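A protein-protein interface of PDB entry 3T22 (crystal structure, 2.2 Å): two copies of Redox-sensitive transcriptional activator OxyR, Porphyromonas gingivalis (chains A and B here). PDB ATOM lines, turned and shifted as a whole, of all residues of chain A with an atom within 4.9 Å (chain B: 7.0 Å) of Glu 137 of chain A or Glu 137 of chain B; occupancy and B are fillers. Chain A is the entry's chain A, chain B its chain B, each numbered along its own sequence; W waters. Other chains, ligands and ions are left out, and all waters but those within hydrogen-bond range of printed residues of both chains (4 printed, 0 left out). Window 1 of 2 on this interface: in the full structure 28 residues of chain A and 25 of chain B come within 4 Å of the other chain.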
ATOM      1  N   PRO A  14     -16.836  -1.722  -8.781  1.00  0.00           N
ATOM      2  CA  PRO A  14     -18.130  -1.858  -8.104  1.00  0.00           C
ATOM      3  C   PRO A  14     -19.163  -0.854  -8.592  1.00  0.00           C
ATOM      4  O   PRO A  14     -20.348  -1.067  -8.376  1.00  0.00           O
ATOM      5  CB  PRO A  14     -17.792  -1.578  -6.626  1.00  0.00           C
ATOM      6  CG  PRO A  14     -16.314  -1.720  -6.522  1.00  0.00           C
ATOM      7  CD  PRO A  14     -15.769  -1.305  -7.854  1.00  0.00           C
ATOM      8  N   TYR A  15     -18.718   0.213  -9.251  1.00  0.00           N
ATOM      9  CA  TYR A  15     -19.609   1.297  -9.635  1.00  0.00           C
ATOM     10  C   TYR A  15     -19.985   1.229 -11.108  1.00  0.00           C
ATOM     11  O   TYR A  15     -21.022   1.753 -11.518  1.00  0.00           O
ATOM     12  CB  TYR A  15     -18.957   2.650  -9.303  1.00  0.00           C
ATOM     13  CG  TYR A  15     -18.249   2.622  -7.973  1.00  0.00           C
ATOM     14  CD1 TYR A  15     -18.946   2.339  -6.807  1.00  0.00           C
ATOM     15  CD2 TYR A  15     -16.892   2.855  -7.884  1.00  0.00           C
ATOM     16  CE1 TYR A  15     -18.313   2.294  -5.591  1.00  0.00           C
ATOM     17  CE2 TYR A  15     -16.246   2.811  -6.669  1.00  0.00           C
ATOM     18  CZ  TYR A  15     -16.958   2.533  -5.531  1.00  0.00           C
ATOM     19  OH  TYR A  15     -16.312   2.486  -4.331  1.00  0.00           O
ATOM     20  N   SER A 135     -10.073  -0.262   2.456  1.00  0.00           N
ATOM     21  CA  SER A 135     -10.950  -0.324   1.293  1.00  0.00           C
ATOM     22  C   SER A 135     -11.968   0.804   1.328  1.00  0.00           C
ATOM     23  O   SER A 135     -12.325   1.314   2.391  1.00  0.00           O
ATOM     24  CB  SER A 135     -11.690  -1.673   1.247  1.00  0.00           C
ATOM     25  OG  SER A 135     -12.545  -1.829   2.367  1.00  0.00           O
ATOM     26  N   MET A 136     -12.430   1.177   0.147  1.00  0.00           N
ATOM     27  CA  MET A 136     -13.462   2.185  -0.041  1.00  0.00           C
ATOM     28  C   MET A 136     -14.719   1.851   0.774  1.00  0.00           C
ATOM     29  O   MET A 136     -15.347   2.745   1.351  1.00  0.00           O
ATOM     30  CB  MET A 136     -13.812   2.281  -1.524  1.00  0.00           C
ATOM     31  CG  MET A 136     -14.786   3.380  -1.855  1.00  0.00           C
ATOM     32  SD  MET A 136     -13.971   4.986  -1.787  1.00  0.00           S
ATOM     33  CE  MET A 136     -12.577   4.642  -2.850  1.00  0.00           C
ATOM     34  N   GLU A 137     -15.086   0.573   0.804  1.00  0.00           N
ATOM     35  CA  GLU A 137     -16.230   0.134   1.600  1.00  0.00           C
ATOM     36  C   GLU A 137     -16.068   0.437   3.089  1.00  0.00           C
ATOM     37  O   GLU A 137     -16.976   0.979   3.722  1.00  0.00           O
ATOM     38  CB  GLU A 137     -16.498  -1.357   1.387  1.00  0.00           C
ATOM     39  CG  GLU A 137     -17.740  -1.876   2.099  1.00  0.00           C
ATOM     40  CD  GLU A 137     -17.701  -3.379   2.289  1.00  0.00           C
ATOM     41  OE1 GLU A 137     -16.600  -3.959   2.234  1.00  0.00           O
ATOM     42  OE2 GLU A 137     -18.769  -3.989   2.485  1.00  0.00           O
ATOM     43  N   ALA A 138     -14.919   0.091   3.652  1.00  0.00           N
ATOM     44  CA  ALA A 138     -14.657   0.388   5.057  1.00  0.00           C
ATOM     45  C   ALA A 138     -14.641   1.894   5.367  1.00  0.00           C
ATOM     46  O   ALA A 138     -15.146   2.315   6.413  1.00  0.00           O
ATOM     47  CB  ALA A 138     -13.355  -0.273   5.518  1.00  0.00           C
ATOM     48  N   PHE A 139     -14.059   2.698   4.469  1.00  0.00           N
ATOM     49  CA  PHE A 139     -14.035   4.141   4.660  1.00  0.00           C
ATOM     50  C   PHE A 139     -15.470   4.685   4.675  1.00  0.00           C
ATOM     51  O   PHE A 139     -15.816   5.481   5.542  1.00  0.00           O
ATOM     52  CB  PHE A 139     -13.213   4.863   3.583  1.00  0.00           C
ATOM     53  CG  PHE A 139     -11.768   4.428   3.502  1.00  0.00           C
ATOM     54  CD1 PHE A 139     -11.106   3.912   4.611  1.00  0.00           C
ATOM     55  CD2 PHE A 139     -11.073   4.523   2.305  1.00  0.00           C
ATOM     56  CE1 PHE A 139      -9.782   3.507   4.522  1.00  0.00           C
ATOM     57  CE2 PHE A 139      -9.759   4.118   2.219  1.00  0.00           C
ATOM     58  CZ  PHE A 139      -9.115   3.607   3.331  1.00  0.00           C
ATOM     59  N   MET A 140     -16.296   4.262   3.719  1.00  0.00           N
ATOM     60  CA  MET A 140     -17.694   4.700   3.680  1.00  0.00           C
ATOM     61  C   MET A 140     -18.481   4.224   4.902  1.00  0.00           C
ATOM     62  O   MET A 140     -19.231   4.998   5.476  1.00  0.00           O
ATOM     63  CB  MET A 140     -18.395   4.295   2.384  1.00  0.00           C
ATOM     64  CG  MET A 140     -17.713   4.844   1.126  1.00  0.00           C
ATOM     65  SD  MET A 140     -18.543   4.398  -0.412  1.00  0.00           S
ATOM     66  CE  MET A 140     -18.865   2.647  -0.152  1.00  0.00           C
ATOM     67  N   ARG A 141     -18.299   2.972   5.323  1.00  0.00           N
ATOM     68  CA  ARG A 141     -18.963   2.526   6.565  1.00  0.00           C
ATOM     69  C   ARG A 141     -18.584   3.410   7.763  1.00  0.00           C
ATOM     70  O   ARG A 141     -19.459   3.834   8.524  1.00  0.00           O
ATOM     71  CB  ARG A 141     -18.756   1.033   6.878  1.00  0.00           C
ATOM     72  CG  ARG A 141     -19.384   0.035   5.872  1.00  0.00           C
ATOM     73  CD  ARG A 141     -20.907   0.196   5.588  1.00  0.00           C
ATOM     74  NE  ARG A 141     -21.207   1.221   4.577  1.00  0.00           N
ATOM     75  CZ  ARG A 141     -21.138   1.050   3.251  1.00  0.00           C
ATOM     76  NH1 ARG A 141     -20.774  -0.118   2.735  1.00  0.00           N
ATOM     77  NH2 ARG A 141     -21.424   2.059   2.426  1.00  0.00           N
ATOM     78  N   PRO B  10      -9.741  -8.165   5.592  1.00  0.00           N
ATOM     79  CA  PRO B  10     -10.536  -7.322   4.681  1.00  0.00           C
ATOM     80  C   PRO B  10     -12.042  -7.609   4.769  1.00  0.00           C
ATOM     81  O   PRO B  10     -12.867  -6.735   4.480  1.00  0.00           O
ATOM     82  CB  PRO B  10     -10.028  -7.724   3.286  1.00  0.00           C
ATOM     83  CG  PRO B  10      -8.703  -8.358   3.512  1.00  0.00           C
ATOM     84  CD  PRO B  10      -8.735  -8.971   4.876  1.00  0.00           C
ATOM     85  N   THR B  11     -12.392  -8.826   5.174  1.00  0.00           N
ATOM     86  CA  THR B  11     -13.791  -9.216   5.305  1.00  0.00           C
ATOM     87  C   THR B  11     -14.337  -9.022   6.738  1.00  0.00           C
ATOM     88  O   THR B  11     -15.400  -9.570   7.085  1.00  0.00           O
ATOM     89  CB  THR B  11     -13.986 -10.695   4.928  1.00  0.00           C
ATOM     90  OG1 THR B  11     -13.417 -11.519   5.944  1.00  0.00           O
ATOM     91  CG2 THR B  11     -13.329 -11.005   3.596  1.00  0.00           C
ATOM     92  N   PRO B  14     -14.594  -3.545   7.565  1.00  0.00           N
ATOM     93  CA  PRO B  14     -15.693  -2.608   7.314  1.00  0.00           C
ATOM     94  C   PRO B  14     -16.829  -2.782   8.329  1.00  0.00           C
ATOM     95  O   PRO B  14     -17.521  -1.821   8.642  1.00  0.00           O
ATOM     96  CB  PRO B  14     -16.210  -3.021   5.934  1.00  0.00           C
ATOM     97  CG  PRO B  14     -15.171  -3.896   5.351  1.00  0.00           C
ATOM     98  CD  PRO B  14     -14.442  -4.530   6.486  1.00  0.00           C
ATOM     99  N   TYR B  15     -17.017  -3.993   8.845  1.00  0.00           N
ATOM    100  CA  TYR B  15     -18.193  -4.264   9.663  1.00  0.00           C
ATOM    101  C   TYR B  15     -17.924  -4.186  11.164  1.00  0.00           C
ATOM    102  O   TYR B  15     -18.817  -3.859  11.940  1.00  0.00           O
ATOM    103  CB  TYR B  15     -18.800  -5.610   9.263  1.00  0.00           C
ATOM    104  CG  TYR B  15     -18.638  -5.873   7.781  1.00  0.00           C
ATOM    105  CD1 TYR B  15     -19.365  -5.138   6.837  1.00  0.00           C
ATOM    106  CD2 TYR B  15     -17.730  -6.819   7.317  1.00  0.00           C
ATOM    107  CE1 TYR B  15     -19.204  -5.359   5.476  1.00  0.00           C
ATOM    108  CE2 TYR B  15     -17.570  -7.054   5.960  1.00  0.00           C
ATOM    109  CZ  TYR B  15     -18.306  -6.323   5.044  1.00  0.00           C
ATOM    110  OH  TYR B  15     -18.133  -6.550   3.696  1.00  0.00           O
ATOM    111  N   LEU B 105     -15.078 -14.648  -3.529  1.00  0.00           N
ATOM    112  CA  LEU B 105     -13.775 -14.013  -3.356  1.00  0.00           C
ATOM    113  C   LEU B 105     -12.655 -14.986  -3.758  1.00  0.00           C
ATOM    114  O   LEU B 105     -12.892 -16.194  -3.896  1.00  0.00           O
ATOM    115  CB  LEU B 105     -13.581 -13.592  -1.908  1.00  0.00           C
ATOM    116  CG  LEU B 105     -14.508 -12.540  -1.302  1.00  0.00           C
ATOM    117  CD1 LEU B 105     -14.301 -12.482   0.202  1.00  0.00           C
ATOM    118  CD2 LEU B 105     -14.312 -11.148  -1.935  1.00  0.00           C
ATOM    119  N   GLY B 134     -12.115  -9.976  -6.969  1.00  0.00           N
ATOM    120  CA  GLY B 134     -13.271  -9.199  -6.545  1.00  0.00           C
ATOM    121  C   GLY B 134     -13.269  -8.728  -5.095  1.00  0.00           C
ATOM    122  O   GLY B 134     -12.658  -9.362  -4.235  1.00  0.00           O
ATOM    123  N   SER B 135     -13.915  -7.592  -4.832  1.00  0.00           N
ATOM    124  CA  SER B 135     -14.214  -7.186  -3.451  1.00  0.00           C
ATOM    125  C   SER B 135     -15.685  -7.448  -3.094  1.00  0.00           C
ATOM    126  O   SER B 135     -16.542  -7.517  -3.970  1.00  0.00           O
ATOM    127  CB  SER B 135     -13.910  -5.711  -3.228  1.00  0.00           C
ATOM    128  OG  SER B 135     -14.779  -4.912  -3.994  1.00  0.00           O
ATOM    129  N   MET B 136     -15.969  -7.585  -1.803  1.00  0.00           N
ATOM    130  CA  MET B 136     -17.333  -7.788  -1.336  1.00  0.00           C
ATOM    131  C   MET B 136     -18.201  -6.607  -1.748  1.00  0.00           C
ATOM    132  O   MET B 136     -19.378  -6.769  -2.058  1.00  0.00           O
ATOM    133  CB  MET B 136     -17.375  -7.924   0.185  1.00  0.00           C
ATOM    134  CG  MET B 136     -18.633  -8.629   0.694  1.00  0.00           C
ATOM    135  SD  MET B 136     -18.193 -10.303   1.222  1.00  0.00           S
ATOM    136  CE  MET B 136     -16.900  -9.919   2.394  1.00  0.00           C
ATOM    137  N   GLU B 137     -17.608  -5.417  -1.749  1.00  0.00           N
ATOM    138  CA  GLU B 137     -18.327  -4.237  -2.208  1.00  0.00           C
ATOM    139  C   GLU B 137     -18.844  -4.438  -3.629  1.00  0.00           C
ATOM    140  O   GLU B 137     -20.030  -4.232  -3.906  1.00  0.00           O
ATOM    141  CB  GLU B 137     -17.445  -3.007  -2.136  1.00  0.00           C
ATOM    142  CG  GLU B 137     -18.149  -1.726  -2.557  1.00  0.00           C
ATOM    143  CD  GLU B 137     -17.175  -0.571  -2.720  1.00  0.00           C
ATOM    144  OE1 GLU B 137     -15.955  -0.805  -2.593  1.00  0.00           O
ATOM    145  OE2 GLU B 137     -17.616   0.571  -2.964  1.00  0.00           O
ATOM    146  N   ALA B 138     -17.957  -4.859  -4.523  1.00  0.00           N
ATOM    147  CA  ALA B 138     -18.356  -5.156  -5.898  1.00  0.00           C
ATOM    148  C   ALA B 138     -19.488  -6.198  -6.012  1.00  0.00           C
ATOM    149  O   ALA B 138     -20.458  -5.998  -6.747  1.00  0.00           O
ATOM    150  CB  ALA B 138     -17.146  -5.577  -6.739  1.00  0.00           C
ATOM    151  N   PHE B 139     -19.352  -7.320  -5.309  1.00  0.00           N
ATOM    152  CA  PHE B 139     -20.340  -8.393  -5.413  1.00  0.00           C
ATOM    153  C   PHE B 139     -21.699  -7.934  -4.928  1.00  0.00           C
ATOM    154  O   PHE B 139     -22.724  -8.236  -5.539  1.00  0.00           O
ATOM    155  CB  PHE B 139     -19.888  -9.608  -4.622  1.00  0.00           C
ATOM    156  CG  PHE B 139     -18.620 -10.202  -5.130  1.00  0.00           C
ATOM    157  CD1 PHE B 139     -18.246 -10.021  -6.450  1.00  0.00           C
ATOM    158  CD2 PHE B 139     -17.785 -10.920  -4.287  1.00  0.00           C
ATOM    159  CE1 PHE B 139     -17.070 -10.578  -6.927  1.00  0.00           C
ATOM    160  CE2 PHE B 139     -16.626 -11.473  -4.755  1.00  0.00           C
ATOM    161  CZ  PHE B 139     -16.265 -11.311  -6.066  1.00  0.00           C
ATOM    162  N   MET B 140     -21.696  -7.191  -3.830  1.00  0.00           N
ATOM    163  CA  MET B 140     -22.941  -6.637  -3.301  1.00  0.00           C
ATOM    164  C   MET B 140     -23.617  -5.703  -4.298  1.00  0.00           C
ATOM    165  O   MET B 140     -24.824  -5.769  -4.492  1.00  0.00           O
ATOM    166  CB  MET B 140     -22.705  -5.941  -1.959  1.00  0.00           C
ATOM    167  CG  MET B 140     -22.354  -6.943  -0.852  1.00  0.00           C
ATOM    168  SD  MET B 140     -22.070  -6.233   0.776  1.00  0.00           S
ATOM    169  CE  MET B 140     -23.721  -5.655   1.188  1.00  0.00           C
ATOM    170  N   ARG B 141     -22.849  -4.838  -4.943  1.00  0.00           N
ATOM    171  CA  ARG B 141     -23.457  -3.887  -5.863  1.00  0.00           C
ATOM    172  C   ARG B 141     -24.070  -4.628  -7.049  1.00  0.00           C
ATOM    173  O   ARG B 141     -25.174  -4.296  -7.504  1.00  0.00           O
ATOM    174  CB  ARG B 141     -22.468  -2.786  -6.303  1.00  0.00           C
ATOM    175  CG  ARG B 141     -22.001  -1.817  -5.176  1.00  0.00           C
ATOM    176  CD  ARG B 141     -23.146  -1.080  -4.446  1.00  0.00           C
ATOM    177  NE  ARG B 141     -23.689  -1.863  -3.323  1.00  0.00           N
ATOM    178  CZ  ARG B 141     -23.097  -1.985  -2.135  1.00  0.00           C
ATOM    179  NH1 ARG B 141     -21.931  -1.391  -1.900  1.00  0.00           N
ATOM    180  NH2 ARG B 141     -23.650  -2.730  -1.185  1.00  0.00           N
ATOM    181  N   LEU B 142     -23.388  -5.676  -7.496  1.00  0.00           N
ATOM    182  CA  LEU B 142     -23.889  -6.534  -8.560  1.00  0.00           C
ATOM    183  C   LEU B 142     -25.231  -7.187  -8.217  1.00  0.00           C
ATOM    184  O   LEU B 142     -26.157  -7.145  -9.014  1.00  0.00           O
ATOM    185  CB  LEU B 142     -22.857  -7.606  -8.913  1.00  0.00           C
ATOM    186  CG  LEU B 142     -21.713  -7.167  -9.826  1.00  0.00           C
ATOM    187  CD1 LEU B 142     -20.621  -8.210  -9.877  1.00  0.00           C
ATOM    188  CD2 LEU B 142     -22.233  -6.877 -11.214  1.00  0.00           C
ATOM    189  N   GLU B 144     -27.471  -6.241  -5.939  1.00  0.00           N
ATOM    190  CA  GLU B 144     -28.495  -5.205  -5.789  1.00  0.00           C
ATOM    191  C   GLU B 144     -28.972  -4.669  -7.145  1.00  0.00           C
ATOM    192  O   GLU B 144     -29.997  -3.986  -7.222  1.00  0.00           O
ATOM    193  CB  GLU B 144     -27.971  -4.042  -4.942  1.00  0.00           C
ATOM    194  CG  GLU B 144     -27.611  -4.436  -3.534  1.00  0.00           C
ATOM    195  CD  GLU B 144     -26.685  -3.452  -2.850  1.00  0.00           C
ATOM    196  OE1 GLU B 144     -26.247  -2.477  -3.498  1.00  0.00           O
ATOM    197  OE2 GLU B 144     -26.402  -3.651  -1.655  1.00  0.00           O
ATOM    198  N   THR B 156     -22.864  -7.386   8.709  1.00  0.00           N
ATOM    199  CA  THR B 156     -23.120  -6.293   7.773  1.00  0.00           C
ATOM    200  C   THR B 156     -24.586  -5.863   7.694  1.00  0.00           C
ATOM    201  O   THR B 156     -24.878  -4.725   7.340  1.00  0.00           O
ATOM    202  CB  THR B 156     -22.625  -6.616   6.354  1.00  0.00           C
ATOM    203  OG1 THR B 156     -23.687  -7.199   5.598  1.00  0.00           O
ATOM    204  CG2 THR B 156     -21.464  -7.578   6.402  1.00  0.00           C
ATOM    205  N   GLN B 159     -25.765  -2.675   8.891  1.00  0.00           N
ATOM    206  CA  GLN B 159     -25.349  -1.510   8.130  1.00  0.00           C
ATOM    207  C   GLN B 159     -26.270  -1.320   6.936  1.00  0.00           C
ATOM    208  O   GLN B 159     -26.206  -0.296   6.267  1.00  0.00           O
ATOM    209  CB  GLN B 159     -23.884  -1.665   7.664  1.00  0.00           C
ATOM    210  CG  GLN B 159     -22.841  -1.698   8.816  1.00  0.00           C
ATOM    211  CD  GLN B 159     -21.395  -1.982   8.342  1.00  0.00           C
ATOM    212  OE1 GLN B 159     -21.171  -2.753   7.405  1.00  0.00           O
ATOM    213  NE2 GLN B 159     -20.421  -1.353   8.999  1.00  0.00           N
HETATM  214  O   HOH W   1     -14.060  -1.756  -1.125  1.00  0.00           O
HETATM  215  O   HOH W   2     -15.318  -4.288  -0.153  1.00  0.00           O
HETATM  216  O   HOH W   3     -12.079  -4.354   3.497  1.00  0.00           O
HETATM  217  O   HOH W   4     -21.512  -2.603   3.936  1.00  0.00           O
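The side-chain hydroxyl (OH) of Tyr 15 of chain A lies within hydrogen-bond range of the side-chain carboxylate (OE2) of Glu 137 of chain B (2.7 Å).
The side-chain carboxylate of Glu 137 of chain A lies within hydrogen-bond range of the side-chain hydroxyl of Tyr 15 of chain B (2.9 Å).
The side-chain hydroxyl (OG) of Ser 135 of chain B is in hydrogen-bond range of the backbone NH (N) of Ala 138 of chain B, 3.2 Å away.
The backbone NH (N) of Ala 138 of chain A lies within hydrogen-bond range of the side-chain hydroxyl (OG) of Ser 135 of chain A, at 3.3 Å.
The guanidinium group of Arg 141 of chain B lies within salt-bridge range of the side-chain carboxylate of Glu 144 of chain B.
The side-chain amide nitrogen (NE2) of Gln 159 of chain B sits at hydrogen-bond distance from the backbone carbonyl oxygen (O) of Pro 14 of chain B (3.0 Å).
Pro 14 of chain A touches Ala 138 of chain B (CB to CA, 3.7 Å).
Arg 141 of chain B touches Pro 14 of chain A.
Glu 137 of chain B touches Met 136 of chain A.
Glu 137 of chain A touches Pro 14 of chain B.
N of Glu 137 of chain A touches OE1 of Glu 137 of chain B, at 3.8 Å.
CB of Ala 138 of chain A touches CA of Pro 14 of chain B (3.8 Å).
CE of Met 140 of chain A touches OE2 of Glu 137 of chain B (3.7 Å).
Arg 141 of chain A touches Pro 14 of chain B (CB to O, 3.6 Å).
Arg 141 of chain A touches Gln 159 of chain B.
Glu 137 of chain A touches just these residues of chain B: Pro 14, Tyr 15 and Glu 137.
Printed residues of chain A within 4 Å of Tyr 15 of chain B: Glu 137 (2.9 Å).
Printed residues of chain A within 4 Å of Ala 138 of chain B: Pro 14 (3.7 Å).
Printed residues of chain A within 4 Å of Gln 159 of chain B: Arg 141.
The nearest residue of chain B that does not touch Glu 137 of chain A is Met 140 of chain B (4.3 Å).
The nearest residue of chain A that does not touch Glu 137 of chain B is Pro 14 of chain A (4.1 Å).
The nearest printed residue of chain A that does not touch Tyr 15 of chain B is Arg 141 of chain A (5.3 Å).
Of the 17 printed residues of chain B, 6 touch a printed residue of chain A.
Of the 9 printed residues of chain A, 7 touch a printed residue of chain B.
Among the printed residues, no Asp or Glu carboxylate lies within 4 Å of a Lys or Arg side-chain nitrogen of the other chain.
Pro 14 of chain A touches Arg 141 of chain B, and with the chains exchanged Arg 141 of chain A touches Pro 14 of chain B.
Met 136 of chain A touches Glu 137 of chain B, but with the chains exchanged Glu 137 of chain A does not touch Met 136 of chain B (4.5 Å).
Glu 137 of chain A touches Pro 14 of chain B, but with the chains exchanged Pro 14 of chain A does not touch Glu 137 of chain B (4.1 Å).
Glu 137 of chain B touches its own counterpart, Glu 137 of chain A.
Of the 11 pairs that touch across the chains among the printed residues, 7 have their exchanged pair printed and touching as well.
Water W1 lies within hydrogen-bond range of the side-chain carboxylate of Glu 137 of chain B (2.6 Å) and the backbone NH of Glu 137 of chain A (3.2 Å).
Water W3 bridges the backbone carbonyl oxygen of Pro 10 of chain B (2.7 Å) and the side-chain hydroxyl of Ser 135 of chain A (2.8 Å).
Water W2 lies within hydrogen-bond range of the side-chain carboxylate of Glu 137 of chain A and the backbone NH of Glu 137 of chain B.
Water W4 lies within hydrogen-bond range of the guanidinium group (NH1) of Arg 141 of chain A, the side-chain carboxylate (OE2) of Glu 137 of chain A and the side-chain amide oxygen (OE1) of Gln 159 of chain B.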
